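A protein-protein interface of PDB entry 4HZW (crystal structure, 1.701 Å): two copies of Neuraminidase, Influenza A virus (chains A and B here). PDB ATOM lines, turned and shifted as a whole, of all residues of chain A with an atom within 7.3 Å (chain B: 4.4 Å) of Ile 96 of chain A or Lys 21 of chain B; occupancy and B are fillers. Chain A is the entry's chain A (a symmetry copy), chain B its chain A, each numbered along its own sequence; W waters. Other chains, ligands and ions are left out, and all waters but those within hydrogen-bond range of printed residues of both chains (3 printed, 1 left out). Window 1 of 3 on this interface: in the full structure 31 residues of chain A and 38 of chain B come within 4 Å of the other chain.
Ile 96 of chain A touches five residues of chain B.
Of the printed residues of chain A, Lys 21 of chain B touches Pro 73, Tyr 74, Ser 76, Glu 93 and Ile 96.
Of the printed residues of chain A, Gly 83 of chain B touches Glu 93.
Of the printed residues of chain A, Trp 377 of chain B touches Pro 73 (3.7 Å), Ile 96 (3.9 Å), Thr 115 (3.1 Å) and Gly 116 (3.6 Å).
Printed residues of chain B within 4 Å of Ile 94 of chain A: His 20 (3.0 Å).
Printed residues of chain A within 4 Å of Pro 18 of chain B: Ile 96, Thr 115 and Gln 124.
Thr 72 of chain A touches none of the printed residues of chain B.
Ala 97 of chain A touches none of the printed residues of chain B.
The nearest residue of chain A that does not touch Lys 21 of chain B is Cys 95 of chain A (5.5 Å).
Of the 12 printed residues of chain B, 8 touch a printed residue of chain A.
Printed residues of chain A that touch a printed residue of chain B: Pro 73, Tyr 74, Ser 76, Glu 93, Ile 94, Cys 95, Ile 96, Thr 115, Gly 116 and Gln 124.
Hydrophobic or aromatic side chains of chain A within 4 Å of the printed part of chain B: Pro 73, Tyr 74 and Ile 96.
Among the printed residues, 20 pairs touch across the chains.
Among the printed residues, no Asp or Glu carboxylate lies within 4 Å of a Lys or Arg side-chain nitrogen of the other chain.
O of Ser 122 of chain A is in hydrogen-bond range of N of Thr 115 of chain A (3.2 Å).
O of Cys 113 of chain A is in hydrogen-bond range of N of Gln 124 of chain A (2.7 Å).
The backbone NH (N) of Leu 77 of chain A is in hydrogen-bond range of the backbone carbonyl oxygen (O) of Cys 95 of chain A, at 2.8 Å.
The side-chain amide oxygen (OE1) of Gln 124 of chain A is in hydrogen-bond range of the side-chain hydroxyl (OG) of Ser 122 of chain A, at 2.7 Å.
N of Ile 94 of chain A lies within hydrogen-bond range of O of Leu 77 of chain A, at 2.8 Å.
O of Asp 379 of chain B is in hydrogen-bond range of NZ of Lys 21 of chain B (3.4 Å).
No position is printed for both chains.
Of the 20 pairs that touch across the chains among the printed residues, none has its exchanged pair printed and touching as well.
Water W2 lies within hydrogen-bond range of the side-chain hydroxyl (OH) of Tyr 91 of chain A, the backbone carbonyl oxygen (O) of Gly 83 of chain B and the backbone carbonyl oxygen (O) of Asp 22 of chain B.
Water W1 lies within hydrogen-bond range of O of Ile 96 of chain A, O of Pro 18 of chain B and NE2 of Gln 124 of chain A.
Water W3 lies within hydrogen-bond range of the side-chain amide oxygen of Asn 23 of chain B (2.9 Å), the side-chain hydroxyl of Ser 76 of chain A (3.1 Å) and the backbone carbonyl oxygen of Lys 21 of chain B (3.2 Å).
Pro 73 of chain A touches Trp 377 of chain B.
Tyr 74 of chain A touches Lys 21 of chain B.
Tyr 74 of chain A touches Pro 378 of chain B.
Ser 76 of chain A touches Lys 21 of chain B (OG to O, 3.6 Å).
His 20 of chain B touches Ile 94 of chain A (CE1 to O, 3.0 Å).
Lys 21 of chain B touches Ile 96 of chain A.
Trp 377 of chain B touches Ile 96 of chain A (NE1 to CG2, 3.9 Å).
Pro 18 of chain B touches Thr 115 of chain A (CG to CG2, 3.5 Å).
Gly 116 of chain A touches Trp 377 of chain B (CA to CZ2, 3.6 Å).
Pro 18 of chain B touches Gln 124 of chain A.
OE1 of Glu 93 of chain A lies within hydrogen-bond range of ND1 of His 20 of chain B (2.6 Å).
O of Phe 19 of chain B is in hydrogen-bond range of N of Ile 96 of chain A.
N of Lys 21 of chain B sits at hydrogen-bond distance from OE2 of Glu 93 of chain A.
NE1 of Trp 377 of chain B sits at hydrogen-bond distance from OG1 of Thr 115 of chain A (3.1 Å).
O of Tyr 74 of chain A sits close to OD1 of Asn 23 of chain B (3.3 Å).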
ATOM      1  N   LEU A  53      27.996  17.720 -13.862  1.00  0.00           N
ATOM      2  CA  LEU A  53      26.967  17.119 -14.699  1.00  0.00           C
ATOM      3  C   LEU A  53      27.605  16.678 -16.008  1.00  0.00           C
ATOM      4  O   LEU A  53      27.962  17.502 -16.846  1.00  0.00           O
ATOM      5  CB  LEU A  53      25.832  18.113 -14.965  1.00  0.00           C
ATOM      6  CG  LEU A  53      25.083  18.599 -13.722  1.00  0.00           C
ATOM      7  CD1 LEU A  53      24.018  19.621 -14.111  1.00  0.00           C
ATOM      8  CD2 LEU A  53      24.455  17.431 -12.951  1.00  0.00           C
ATOM      9  N   THR A  72      19.422  16.941 -21.127  1.00  0.00           N
ATOM     10  CA  THR A  72      19.196  15.740 -21.919  1.00  0.00           C
ATOM     11  C   THR A  72      19.092  14.572 -20.950  1.00  0.00           C
ATOM     12  O   THR A  72      19.519  14.679 -19.801  1.00  0.00           O
ATOM     13  CB  THR A  72      20.356  15.445 -22.904  1.00  0.00           C
ATOM     14  OG1 THR A  72      21.391  14.724 -22.226  1.00  0.00           O
ATOM     15  CG2 THR A  72      20.920  16.724 -23.496  1.00  0.00           C
ATOM     16  N   PRO A  73      18.540  13.447 -21.416  1.00  0.00           N
ATOM     17  CA  PRO A  73      18.431  12.241 -20.590  1.00  0.00           C
ATOM     18  C   PRO A  73      19.794  11.591 -20.364  1.00  0.00           C
ATOM     19  O   PRO A  73      19.909  10.695 -19.530  1.00  0.00           O
ATOM     20  CB  PRO A  73      17.558  11.307 -21.440  1.00  0.00           C
ATOM     21  CG  PRO A  73      16.947  12.169 -22.502  1.00  0.00           C
ATOM     22  CD  PRO A  73      17.929  13.271 -22.742  1.00  0.00           C
ATOM     23  N   TYR A  74      20.808  12.048 -21.094  1.00  0.00           N
ATOM     24  CA  TYR A  74      22.125  11.418 -21.080  1.00  0.00           C
ATOM     25  C   TYR A  74      23.064  12.127 -20.118  1.00  0.00           C
ATOM     26  O   TYR A  74      24.256  11.830 -20.072  1.00  0.00           O
ATOM     27  CB  TYR A  74      22.708  11.402 -22.498  1.00  0.00           C
ATOM     28  CG  TYR A  74      21.634  11.079 -23.503  1.00  0.00           C
ATOM     29  CD1 TYR A  74      20.911   9.900 -23.395  1.00  0.00           C
ATOM     30  CD2 TYR A  74      21.310  11.963 -24.526  1.00  0.00           C
ATOM     31  CE1 TYR A  74      19.897   9.601 -24.285  1.00  0.00           C
ATOM     32  CE2 TYR A  74      20.298  11.669 -25.429  1.00  0.00           C
ATOM     33  CZ  TYR A  74      19.597  10.483 -25.300  1.00  0.00           C
ATOM     34  OH  TYR A  74      18.586  10.167 -26.182  1.00  0.00           O
ATOM     35  N   ARG A  75      22.520  13.071 -19.358  1.00  0.00           N
ATOM     36  CA  ARG A  75      23.305  13.745 -18.337  1.00  0.00           C
ATOM     37  C   ARG A  75      23.162  13.046 -16.996  1.00  0.00           C
ATOM     38  O   ARG A  75      22.056  12.690 -16.576  1.00  0.00           O
ATOM     39  CB  ARG A  75      22.903  15.217 -18.219  1.00  0.00           C
ATOM     40  CG  ARG A  75      23.082  15.991 -19.518  1.00  0.00           C
ATOM     41  CD  ARG A  75      23.225  17.477 -19.253  1.00  0.00           C
ATOM     42  NE  ARG A  75      24.547  17.819 -18.743  1.00  0.00           N
ATOM     43  CZ  ARG A  75      24.944  19.067 -18.529  1.00  0.00           C
ATOM     44  NH1 ARG A  75      24.117  20.072 -18.786  1.00  0.00           N
ATOM     45  NH2 ARG A  75      26.167  19.315 -18.073  1.00  0.00           N
ATOM     46  N   SER A  76      24.301  12.859 -16.334  1.00  0.00           N
ATOM     47  CA  SER A  76      24.370  12.272 -15.008  1.00  0.00           C
ATOM     48  C   SER A  76      25.246  13.124 -14.107  1.00  0.00           C
ATOM     49  O   SER A  76      26.227  13.713 -14.565  1.00  0.00           O
ATOM     50  CB  SER A  76      24.998  10.880 -15.075  1.00  0.00           C
ATOM     51  OG  SER A  76      24.113   9.939 -15.660  1.00  0.00           O
ATOM     52  N   LEU A  77      24.907  13.171 -12.824  1.00  0.00           N
ATOM     53  CA  LEU A  77      25.840  13.702 -11.847  1.00  0.00           C
ATOM     54  C   LEU A  77      26.955  12.675 -11.694  1.00  0.00           C
ATOM     55  O   LEU A  77      26.690  11.503 -11.426  1.00  0.00           O
ATOM     56  CB  LEU A  77      25.147  13.936 -10.506  1.00  0.00           C
ATOM     57  CG  LEU A  77      26.053  14.356  -9.347  1.00  0.00           C
ATOM     58  CD1 LEU A  77      26.717  15.725  -9.626  1.00  0.00           C
ATOM     59  CD2 LEU A  77      25.256  14.396  -8.057  1.00  0.00           C
ATOM     60  N   TYR A  91      35.837   7.827 -12.665  1.00  0.00           N
ATOM     61  CA  TYR A  91      34.574   8.421 -12.244  1.00  0.00           C
ATOM     62  C   TYR A  91      33.599   7.461 -11.573  1.00  0.00           C
ATOM     63  O   TYR A  91      33.681   6.236 -11.736  1.00  0.00           O
ATOM     64  CB  TYR A  91      33.891   9.152 -13.406  1.00  0.00           C
ATOM     65  CG  TYR A  91      33.058   8.308 -14.360  1.00  0.00           C
ATOM     66  CD1 TYR A  91      31.742   8.653 -14.643  1.00  0.00           C
ATOM     67  CD2 TYR A  91      33.591   7.196 -14.998  1.00  0.00           C
ATOM     68  CE1 TYR A  91      30.970   7.910 -15.533  1.00  0.00           C
ATOM     69  CE2 TYR A  91      32.824   6.442 -15.894  1.00  0.00           C
ATOM     70  CZ  TYR A  91      31.518   6.808 -16.155  1.00  0.00           C
ATOM     71  OH  TYR A  91      30.758   6.076 -17.047  1.00  0.00           O
ATOM     72  N   GLU A  93      29.258   7.309 -11.120  1.00  0.00           N
ATOM     73  CA  GLU A  93      27.997   7.921 -11.512  1.00  0.00           C
ATOM     74  C   GLU A  93      27.090   7.940 -10.291  1.00  0.00           C
ATOM     75  O   GLU A  93      26.845   6.906  -9.672  1.00  0.00           O
ATOM     76  CB  GLU A  93      27.348   7.134 -12.651  1.00  0.00           C
ATOM     77  CG  GLU A  93      26.263   7.921 -13.408  1.00  0.00           C
ATOM     78  CD  GLU A  93      24.866   7.368 -13.217  1.00  0.00           C
ATOM     79  OE1 GLU A  93      24.705   6.367 -12.498  1.00  0.00           O
ATOM     80  OE2 GLU A  93      23.919   7.946 -13.792  1.00  0.00           O
ATOM     81  N   ILE A  94      26.608   9.123  -9.929  1.00  0.00           N
ATOM     82  CA  ILE A  94      25.825   9.272  -8.709  1.00  0.00           C
ATOM     83  C   ILE A  94      24.341   9.072  -9.000  1.00  0.00           C
ATOM     84  O   ILE A  94      23.645   8.367  -8.272  1.00  0.00           O
ATOM     85  CB  ILE A  94      26.050  10.657  -8.063  1.00  0.00           C
ATOM     86  CG1 ILE A  94      27.542  10.892  -7.809  1.00  0.00           C
ATOM     87  CG2 ILE A  94      25.268  10.774  -6.755  1.00  0.00           C
ATOM     88  CD1 ILE A  94      28.156   9.868  -6.878  1.00  0.00           C
ATOM     89  N   CYS A  95      23.867   9.698 -10.070  1.00  0.00           N
ATOM     90  CA  CYS A  95      22.461   9.624 -10.444  1.00  0.00           C
ATOM     91  C   CYS A  95      22.248  10.300 -11.789  1.00  0.00           C
ATOM     92  O   CYS A  95      23.080  11.088 -12.243  1.00  0.00           O
ATOM     93  CB  CYS A  95      21.611  10.344  -9.406  1.00  0.00           C
ATOM     94  SG  CYS A  95      22.123  12.076  -9.213  1.00  0.00           S
ATOM     95  N   ILE A  96      21.117  10.003 -12.416  1.00  0.00           N
ATOM     96  CA  ILE A  96      20.728  10.693 -13.639  1.00  0.00           C
ATOM     97  C   ILE A  96      20.297  12.100 -13.252  1.00  0.00           C
ATOM     98  O   ILE A  96      19.476  12.264 -12.360  1.00  0.00           O
ATOM     99  CB  ILE A  96      19.550   9.983 -14.305  1.00  0.00           C
ATOM    100  CG1 ILE A  96      19.883   8.499 -14.530  1.00  0.00           C
ATOM    101  CG2 ILE A  96      19.199  10.681 -15.605  1.00  0.00           C
ATOM    102  CD1 ILE A  96      18.680   7.644 -14.910  1.00  0.00           C
ATOM    103  N   ALA A  97      20.836  13.114 -13.919  1.00  0.00           N
ATOM    104  CA  ALA A  97      20.575  14.491 -13.503  1.00  0.00           C
ATOM    105  C   ALA A  97      21.030  15.523 -14.524  1.00  0.00           C
ATOM    106  O   ALA A  97      22.138  15.427 -15.055  1.00  0.00           O
ATOM    107  CB  ALA A  97      21.259  14.764 -12.163  1.00  0.00           C
ATOM    108  N   TRP A  98      20.182  16.521 -14.784  1.00  0.00           N
ATOM    109  CA  TRP A  98      20.630  17.723 -15.489  1.00  0.00           C
ATOM    110  C   TRP A  98      20.630  18.967 -14.588  1.00  0.00           C
ATOM    111  O   TRP A  98      20.864  20.084 -15.048  1.00  0.00           O
ATOM    112  CB  TRP A  98      19.891  17.963 -16.820  1.00  0.00           C
ATOM    113  CG  TRP A  98      18.392  17.743 -16.843  1.00  0.00           C
ATOM    114  CD1 TRP A  98      17.723  16.795 -17.562  1.00  0.00           C
ATOM    115  CD2 TRP A  98      17.384  18.516 -16.168  1.00  0.00           C
ATOM    116  NE1 TRP A  98      16.367  16.915 -17.365  1.00  0.00           N
ATOM    117  CE2 TRP A  98      16.133  17.961 -16.510  1.00  0.00           C
ATOM    118  CE3 TRP A  98      17.421  19.615 -15.304  1.00  0.00           C
ATOM    119  CZ2 TRP A  98      14.926  18.465 -16.014  1.00  0.00           C
ATOM    120  CZ3 TRP A  98      16.220  20.118 -14.810  1.00  0.00           C
ATOM    121  CH2 TRP A  98      14.991  19.544 -15.166  1.00  0.00           C
ATOM    122  N   SER A  99      20.372  18.751 -13.302  1.00  0.00           N
ATOM    123  CA  SER A  99      20.564  19.759 -12.264  1.00  0.00           C
ATOM    124  C   SER A  99      20.769  18.984 -10.977  1.00  0.00           C
ATOM    125  O   SER A  99      20.148  17.935 -10.786  1.00  0.00           O
ATOM    126  CB  SER A  99      19.337  20.664 -12.138  1.00  0.00           C
ATOM    127  OG  SER A  99      19.554  21.665 -11.153  1.00  0.00           O
ATOM    128  N   SER A 100      21.641  19.470 -10.097  1.00  0.00           N
ATOM    129  CA  SER A 100      21.976  18.693  -8.902  1.00  0.00           C
ATOM    130  C   SER A 100      22.522  19.489  -7.733  1.00  0.00           C
ATOM    131  O   SER A 100      22.937  20.640  -7.871  1.00  0.00           O
ATOM    132  CB  SER A 100      22.983  17.585  -9.250  1.00  0.00           C
ATOM    133  OG  SER A 100      24.317  18.081  -9.203  1.00  0.00           O
ATOM    134  N   VAL A 112      20.697  15.454  -4.634  1.00  0.00           N
ATOM    135  CA  VAL A 112      19.422  15.860  -5.204  1.00  0.00           C
ATOM    136  C   VAL A 112      19.625  15.907  -6.712  1.00  0.00           C
ATOM    137  O   VAL A 112      20.481  16.653  -7.205  1.00  0.00           O
ATOM    138  CB  VAL A 112      19.008  17.258  -4.702  1.00  0.00           C
ATOM    139  CG1 VAL A 112      17.621  17.623  -5.210  1.00  0.00           C
ATOM    140  CG2 VAL A 112      19.054  17.321  -3.171  1.00  0.00           C
ATOM    141  N   CYS A 113      18.854  15.106  -7.444  1.00  0.00           N
ATOM    142  CA  CYS A 113      19.067  14.931  -8.880  1.00  0.00           C
ATOM    143  C   CYS A 113      17.786  15.167  -9.676  1.00  0.00           C
ATOM    144  O   CYS A 113      16.829  14.405  -9.542  1.00  0.00           O
ATOM    145  CB  CYS A 113      19.553  13.506  -9.142  1.00  0.00           C
ATOM    146  SG  CYS A 113      20.818  12.966  -7.952  1.00  0.00           S
ATOM    147  N   MET A 114      17.772  16.203 -10.513  1.00  0.00           N
ATOM    148  CA  MET A 114      16.604  16.477 -11.355  1.00  0.00           C
ATOM    149  C   MET A 114      16.795  15.907 -12.746  1.00  0.00           C
ATOM    150  O   MET A 114      17.851  16.089 -13.347  1.00  0.00           O
ATOM    151  CB  MET A 114      16.356  17.980 -11.488  1.00  0.00           C
ATOM    152  CG  MET A 114      15.597  18.596 -10.334  1.00  0.00           C
ATOM    153  SD  MET A 114      16.690  18.850  -8.948  1.00  0.00           S
ATOM    154  CE  MET A 114      15.664  19.909  -7.919  1.00  0.00           C
ATOM    155  N   THR A 115      15.781  15.223 -13.265  1.00  0.00           N
ATOM    156  CA  THR A 115      15.827  14.777 -14.654  1.00  0.00           C
ATOM    157  C   THR A 115      14.402  14.593 -15.166  1.00  0.00           C
ATOM    158  O   THR A 115      13.440  14.709 -14.401  1.00  0.00           O
ATOM    159  CB  THR A 115      16.671  13.482 -14.834  1.00  0.00           C
ATOM    160  OG1 THR A 115      16.800  13.163 -16.233  1.00  0.00           O
ATOM    161  CG2 THR A 115      16.031  12.320 -14.102  1.00  0.00           C
ATOM    162  N   GLY A 116      14.275  14.334 -16.460  1.00  0.00           N
ATOM    163  CA  GLY A 116      12.974  14.192 -17.087  1.00  0.00           C
ATOM    164  C   GLY A 116      12.599  15.382 -17.952  1.00  0.00           C
ATOM    165  O   GLY A 116      13.405  16.282 -18.170  1.00  0.00           O
ATOM    166  N   SER A 122      11.296  15.477 -12.120  1.00  0.00           N
ATOM    167  CA  SER A 122      11.283  15.130 -10.706  1.00  0.00           C
ATOM    168  C   SER A 122      12.706  15.138 -10.186  1.00  0.00           C
ATOM    169  O   SER A 122      13.653  14.894 -10.938  1.00  0.00           O
ATOM    170  CB  SER A 122      10.642  13.757 -10.464  1.00  0.00           C
ATOM    171  OG  SER A 122      11.348  12.735 -11.145  1.00  0.00           O
ATOM    172  N   GLN A 124      15.228  13.359  -7.589  1.00  0.00           N
ATOM    173  CA  GLN A 124      15.412  12.172  -6.783  1.00  0.00           C
ATOM    174  C   GLN A 124      16.345  12.501  -5.638  1.00  0.00           C
ATOM    175  O   GLN A 124      17.385  13.130  -5.838  1.00  0.00           O
ATOM    176  CB  GLN A 124      15.971  11.029  -7.634  1.00  0.00           C
ATOM    177  CG  GLN A 124      14.942  10.406  -8.578  1.00  0.00           C
ATOM    178  CD  GLN A 124      14.294  11.430  -9.497  1.00  0.00           C
ATOM    179  OE1 GLN A 124      13.096  11.698  -9.397  1.00  0.00           O
ATOM    180  NE2 GLN A 124      15.083  12.010 -10.393  1.00  0.00           N
ATOM    181  N   ILE A 126      18.876  11.021  -3.011  1.00  0.00           N
ATOM    182  CA  ILE A 126      19.715   9.850  -2.769  1.00  0.00           C
ATOM    183  C   ILE A 126      20.423  10.057  -1.441  1.00  0.00           C
ATOM    184  O   ILE A 126      20.951  11.140  -1.179  1.00  0.00           O
ATOM    185  CB  ILE A 126      20.804   9.680  -3.853  1.00  0.00           C
ATOM    186  CG1 ILE A 126      20.231   9.872  -5.262  1.00  0.00           C
ATOM    187  CG2 ILE A 126      21.512   8.325  -3.700  1.00  0.00           C
ATOM    188  CD1 ILE A 126      19.126   8.904  -5.631  1.00  0.00           C
ATOM    189  N   PRO B  18      13.822   7.591 -12.069  1.00  0.00           N
ATOM    190  CA  PRO B  18      15.132   7.347 -12.692  1.00  0.00           C
ATOM    191  C   PRO B  18      16.259   7.410 -11.675  1.00  0.00           C
ATOM    192  O   PRO B  18      16.333   8.357 -10.887  1.00  0.00           O
ATOM    193  CB  PRO B  18      15.284   8.490 -13.701  1.00  0.00           C
ATOM    194  CG  PRO B  18      14.200   9.469 -13.415  1.00  0.00           C
ATOM    195  CD  PRO B  18      13.286   8.932 -12.362  1.00  0.00           C
ATOM    196  N   PHE B  19      17.140   6.417 -11.726  1.00  0.00           N
ATOM    197  CA  PHE B  19      18.158   6.203 -10.702  1.00  0.00           C
ATOM    198  C   PHE B  19      19.548   6.434 -11.309  1.00  0.00           C
ATOM    199  O   PHE B  19      20.094   7.551 -11.242  1.00  0.00           O
ATOM    200  CB  PHE B  19      17.984   4.771 -10.168  1.00  0.00           C
ATOM    201  CG  PHE B  19      18.762   4.452  -8.910  1.00  0.00           C
ATOM    202  CD1 PHE B  19      19.199   5.444  -8.052  1.00  0.00           C
ATOM    203  CD2 PHE B  19      19.018   3.127  -8.576  1.00  0.00           C
ATOM    204  CE1 PHE B  19      19.905   5.121  -6.894  1.00  0.00           C
ATOM    205  CE2 PHE B  19      19.717   2.799  -7.423  1.00  0.00           C
ATOM    206  CZ  PHE B  19      20.156   3.804  -6.581  1.00  0.00           C
ATOM    207  N   HIS B  20      20.101   5.389 -11.924  1.00  0.00           N
ATOM    208  CA  HIS B  20      21.418   5.433 -12.562  1.00  0.00           C
ATOM    209  C   HIS B  20      21.301   5.133 -14.065  1.00  0.00           C
ATOM    210  O   HIS B  20      20.470   4.323 -14.476  1.00  0.00           O
ATOM    211  CB  HIS B  20      22.344   4.376 -11.950  1.00  0.00           C
ATOM    212  CG  HIS B  20      22.784   4.658 -10.543  1.00  0.00           C
ATOM    213  ND1 HIS B  20      23.906   5.410 -10.251  1.00  0.00           N
ATOM    214  CD2 HIS B  20      22.297   4.235  -9.355  1.00  0.00           C
ATOM    215  CE1 HIS B  20      24.068   5.461  -8.941  1.00  0.00           C
ATOM    216  NE2 HIS B  20      23.106   4.756  -8.371  1.00  0.00           N
ATOM    217  N   LYS B  21      22.152   5.748 -14.879  1.00  0.00           N
ATOM    218  CA  LYS B  21      22.176   5.464 -16.320  1.00  0.00           C
ATOM    219  C   LYS B  21      23.615   5.509 -16.816  1.00  0.00           C
ATOM    220  O   LYS B  21      24.321   6.476 -16.555  1.00  0.00           O
ATOM    221  CB  LYS B  21      21.344   6.494 -17.088  1.00  0.00           C
ATOM    222  CG  LYS B  21      21.143   6.158 -18.560  1.00  0.00           C
ATOM    223  CD  LYS B  21      20.371   7.269 -19.267  1.00  0.00           C
ATOM    224  CE  LYS B  21      19.988   6.865 -20.685  1.00  0.00           C
ATOM    225  NZ  LYS B  21      21.159   6.460 -21.514  1.00  0.00           N
ATOM    226  N   ASP B  22      24.069   4.483 -17.533  1.00  0.00           N
ATOM    227  CA  ASP B  22      25.496   4.463 -17.859  1.00  0.00           C
ATOM    228  C   ASP B  22      25.915   5.040 -19.222  1.00  0.00           C
ATOM    229  O   ASP B  22      27.083   5.389 -19.404  1.00  0.00           O
ATOM    230  CB  ASP B  22      26.134   3.091 -17.588  1.00  0.00           C
ATOM    231  CG  ASP B  22      25.660   2.014 -18.537  1.00  0.00           C
ATOM    232  OD1 ASP B  22      25.070   2.337 -19.586  1.00  0.00           O
ATOM    233  OD2 ASP B  22      25.913   0.823 -18.238  1.00  0.00           O
ATOM    234  N   ASN B  23      24.980   5.166 -20.161  1.00  0.00           N
ATOM    235  CA  ASN B  23      25.310   5.771 -21.451  1.00  0.00           C
ATOM    236  C   ASN B  23      26.522   5.073 -22.073  1.00  0.00           C
ATOM    237  O   ASN B  23      27.339   5.700 -22.744  1.00  0.00           O
ATOM    238  CB  ASN B  23      25.605   7.274 -21.267  1.00  0.00           C
ATOM    239  CG  ASN B  23      24.417   8.042 -20.714  1.00  0.00           C
ATOM    240  OD1 ASN B  23      24.463   8.581 -19.599  1.00  0.00           O
ATOM    241  ND2 ASN B  23      23.345   8.100 -21.486  1.00  0.00           N
ATOM    242  N   GLY B  83      26.077   2.483 -12.964  1.00  0.00           N
ATOM    243  CA  GLY B  83      25.924   3.683 -13.758  1.00  0.00           C
ATOM    244  C   GLY B  83      27.180   4.130 -14.479  1.00  0.00           C
ATOM    245  O   GLY B  83      27.158   5.150 -15.161  1.00  0.00           O
ATOM    246  N   ILE B 362      22.732   0.547 -19.958  1.00  0.00           N
ATOM    247  CA  ILE B 362      21.838   0.234 -18.848  1.00  0.00           C
ATOM    248  C   ILE B 362      21.147   1.500 -18.363  1.00  0.00           C
ATOM    249  O   ILE B 362      21.749   2.575 -18.333  1.00  0.00           O
ATOM    250  CB  ILE B 362      22.622  -0.367 -17.656  1.00  0.00           C
ATOM    251  CG1 ILE B 362      23.464  -1.566 -18.103  1.00  0.00           C
ATOM    252  CG2 ILE B 362      21.670  -0.786 -16.532  1.00  0.00           C
ATOM    253  CD1 ILE B 362      24.339  -2.143 -16.996  1.00  0.00           C
ATOM    254  N   VAL B 363      19.879   1.376 -17.989  1.00  0.00           N
ATOM    255  CA  VAL B 363      19.211   2.428 -17.231  1.00  0.00           C
ATOM    256  C   VAL B 363      18.463   1.755 -16.080  1.00  0.00           C
ATOM    257  O   VAL B 363      18.046   0.603 -16.199  1.00  0.00           O
ATOM    258  CB  VAL B 363      18.267   3.282 -18.113  1.00  0.00           C
ATOM    259  CG1 VAL B 363      17.146   2.430 -18.699  1.00  0.00           C
ATOM    260  CG2 VAL B 363      17.712   4.455 -17.325  1.00  0.00           C
ATOM    261  N   TRP B 377      14.400   7.893 -21.255  1.00  0.00           N
ATOM    262  CA  TRP B 377      15.821   7.650 -20.994  1.00  0.00           C
ATOM    263  C   TRP B 377      16.332   6.461 -21.801  1.00  0.00           C
ATOM    264  O   TRP B 377      16.625   5.406 -21.248  1.00  0.00           O
ATOM    265  CB  TRP B 377      16.075   7.433 -19.497  1.00  0.00           C
ATOM    266  CG  TRP B 377      15.702   8.617 -18.650  1.00  0.00           C
ATOM    267  CD1 TRP B 377      16.507   9.664 -18.299  1.00  0.00           C
ATOM    268  CD2 TRP B 377      14.419   8.880 -18.059  1.00  0.00           C
ATOM    269  NE1 TRP B 377      15.804  10.563 -17.525  1.00  0.00           N
ATOM    270  CE2 TRP B 377      14.522  10.100 -17.360  1.00  0.00           C
ATOM    271  CE3 TRP B 377      13.195   8.196 -18.051  1.00  0.00           C
ATOM    272  CZ2 TRP B 377      13.451  10.653 -16.654  1.00  0.00           C
ATOM    273  CZ3 TRP B 377      12.131   8.745 -17.349  1.00  0.00           C
ATOM    274  CH2 TRP B 377      12.264   9.965 -16.660  1.00  0.00           C
ATOM    275  N   PRO B 378      16.439   6.636 -23.125  1.00  0.00           N
ATOM    276  CA  PRO B 378      16.887   5.574 -24.027  1.00  0.00           C
ATOM    277  C   PRO B 378      18.408   5.525 -24.091  1.00  0.00           C
ATOM    278  O   PRO B 378      19.069   6.322 -23.431  1.00  0.00           O
ATOM    279  CB  PRO B 378      16.326   6.023 -25.372  1.00  0.00           C
ATOM    280  CG  PRO B 378      16.415   7.525 -25.297  1.00  0.00           C
ATOM    281  CD  PRO B 378      16.213   7.903 -23.842  1.00  0.00           C
ATOM    282  N   ASP B 379      18.948   4.604 -24.885  1.00  0.00           N
ATOM    283  CA  ASP B 379      20.395   4.462 -25.016  1.00  0.00           C
ATOM    284  C   ASP B 379      21.060   5.783 -25.397  1.00  0.00           C
ATOM    285  O   ASP B 379      22.064   6.182 -24.805  1.00  0.00           O
ATOM    286  CB  ASP B 379      20.720   3.407 -26.064  1.00  0.00           C
ATOM    287  CG  ASP B 379      22.194   3.326 -26.357  1.00  0.00           C
ATOM    288  OD1 ASP B 379      22.950   2.864 -25.479  1.00  0.00           O
ATOM    289  OD2 ASP B 379      22.591   3.729 -27.463  1.00  0.00           O
HETATM  290  O   HOH W   1      17.836  10.851 -10.607  1.00  0.00           O
HETATM  291  O   HOH W   2      28.163   6.661 -17.173  1.00  0.00           O
HETATM  292  O   HOH W   3      26.360   8.791 -17.384  1.00  0.00           O
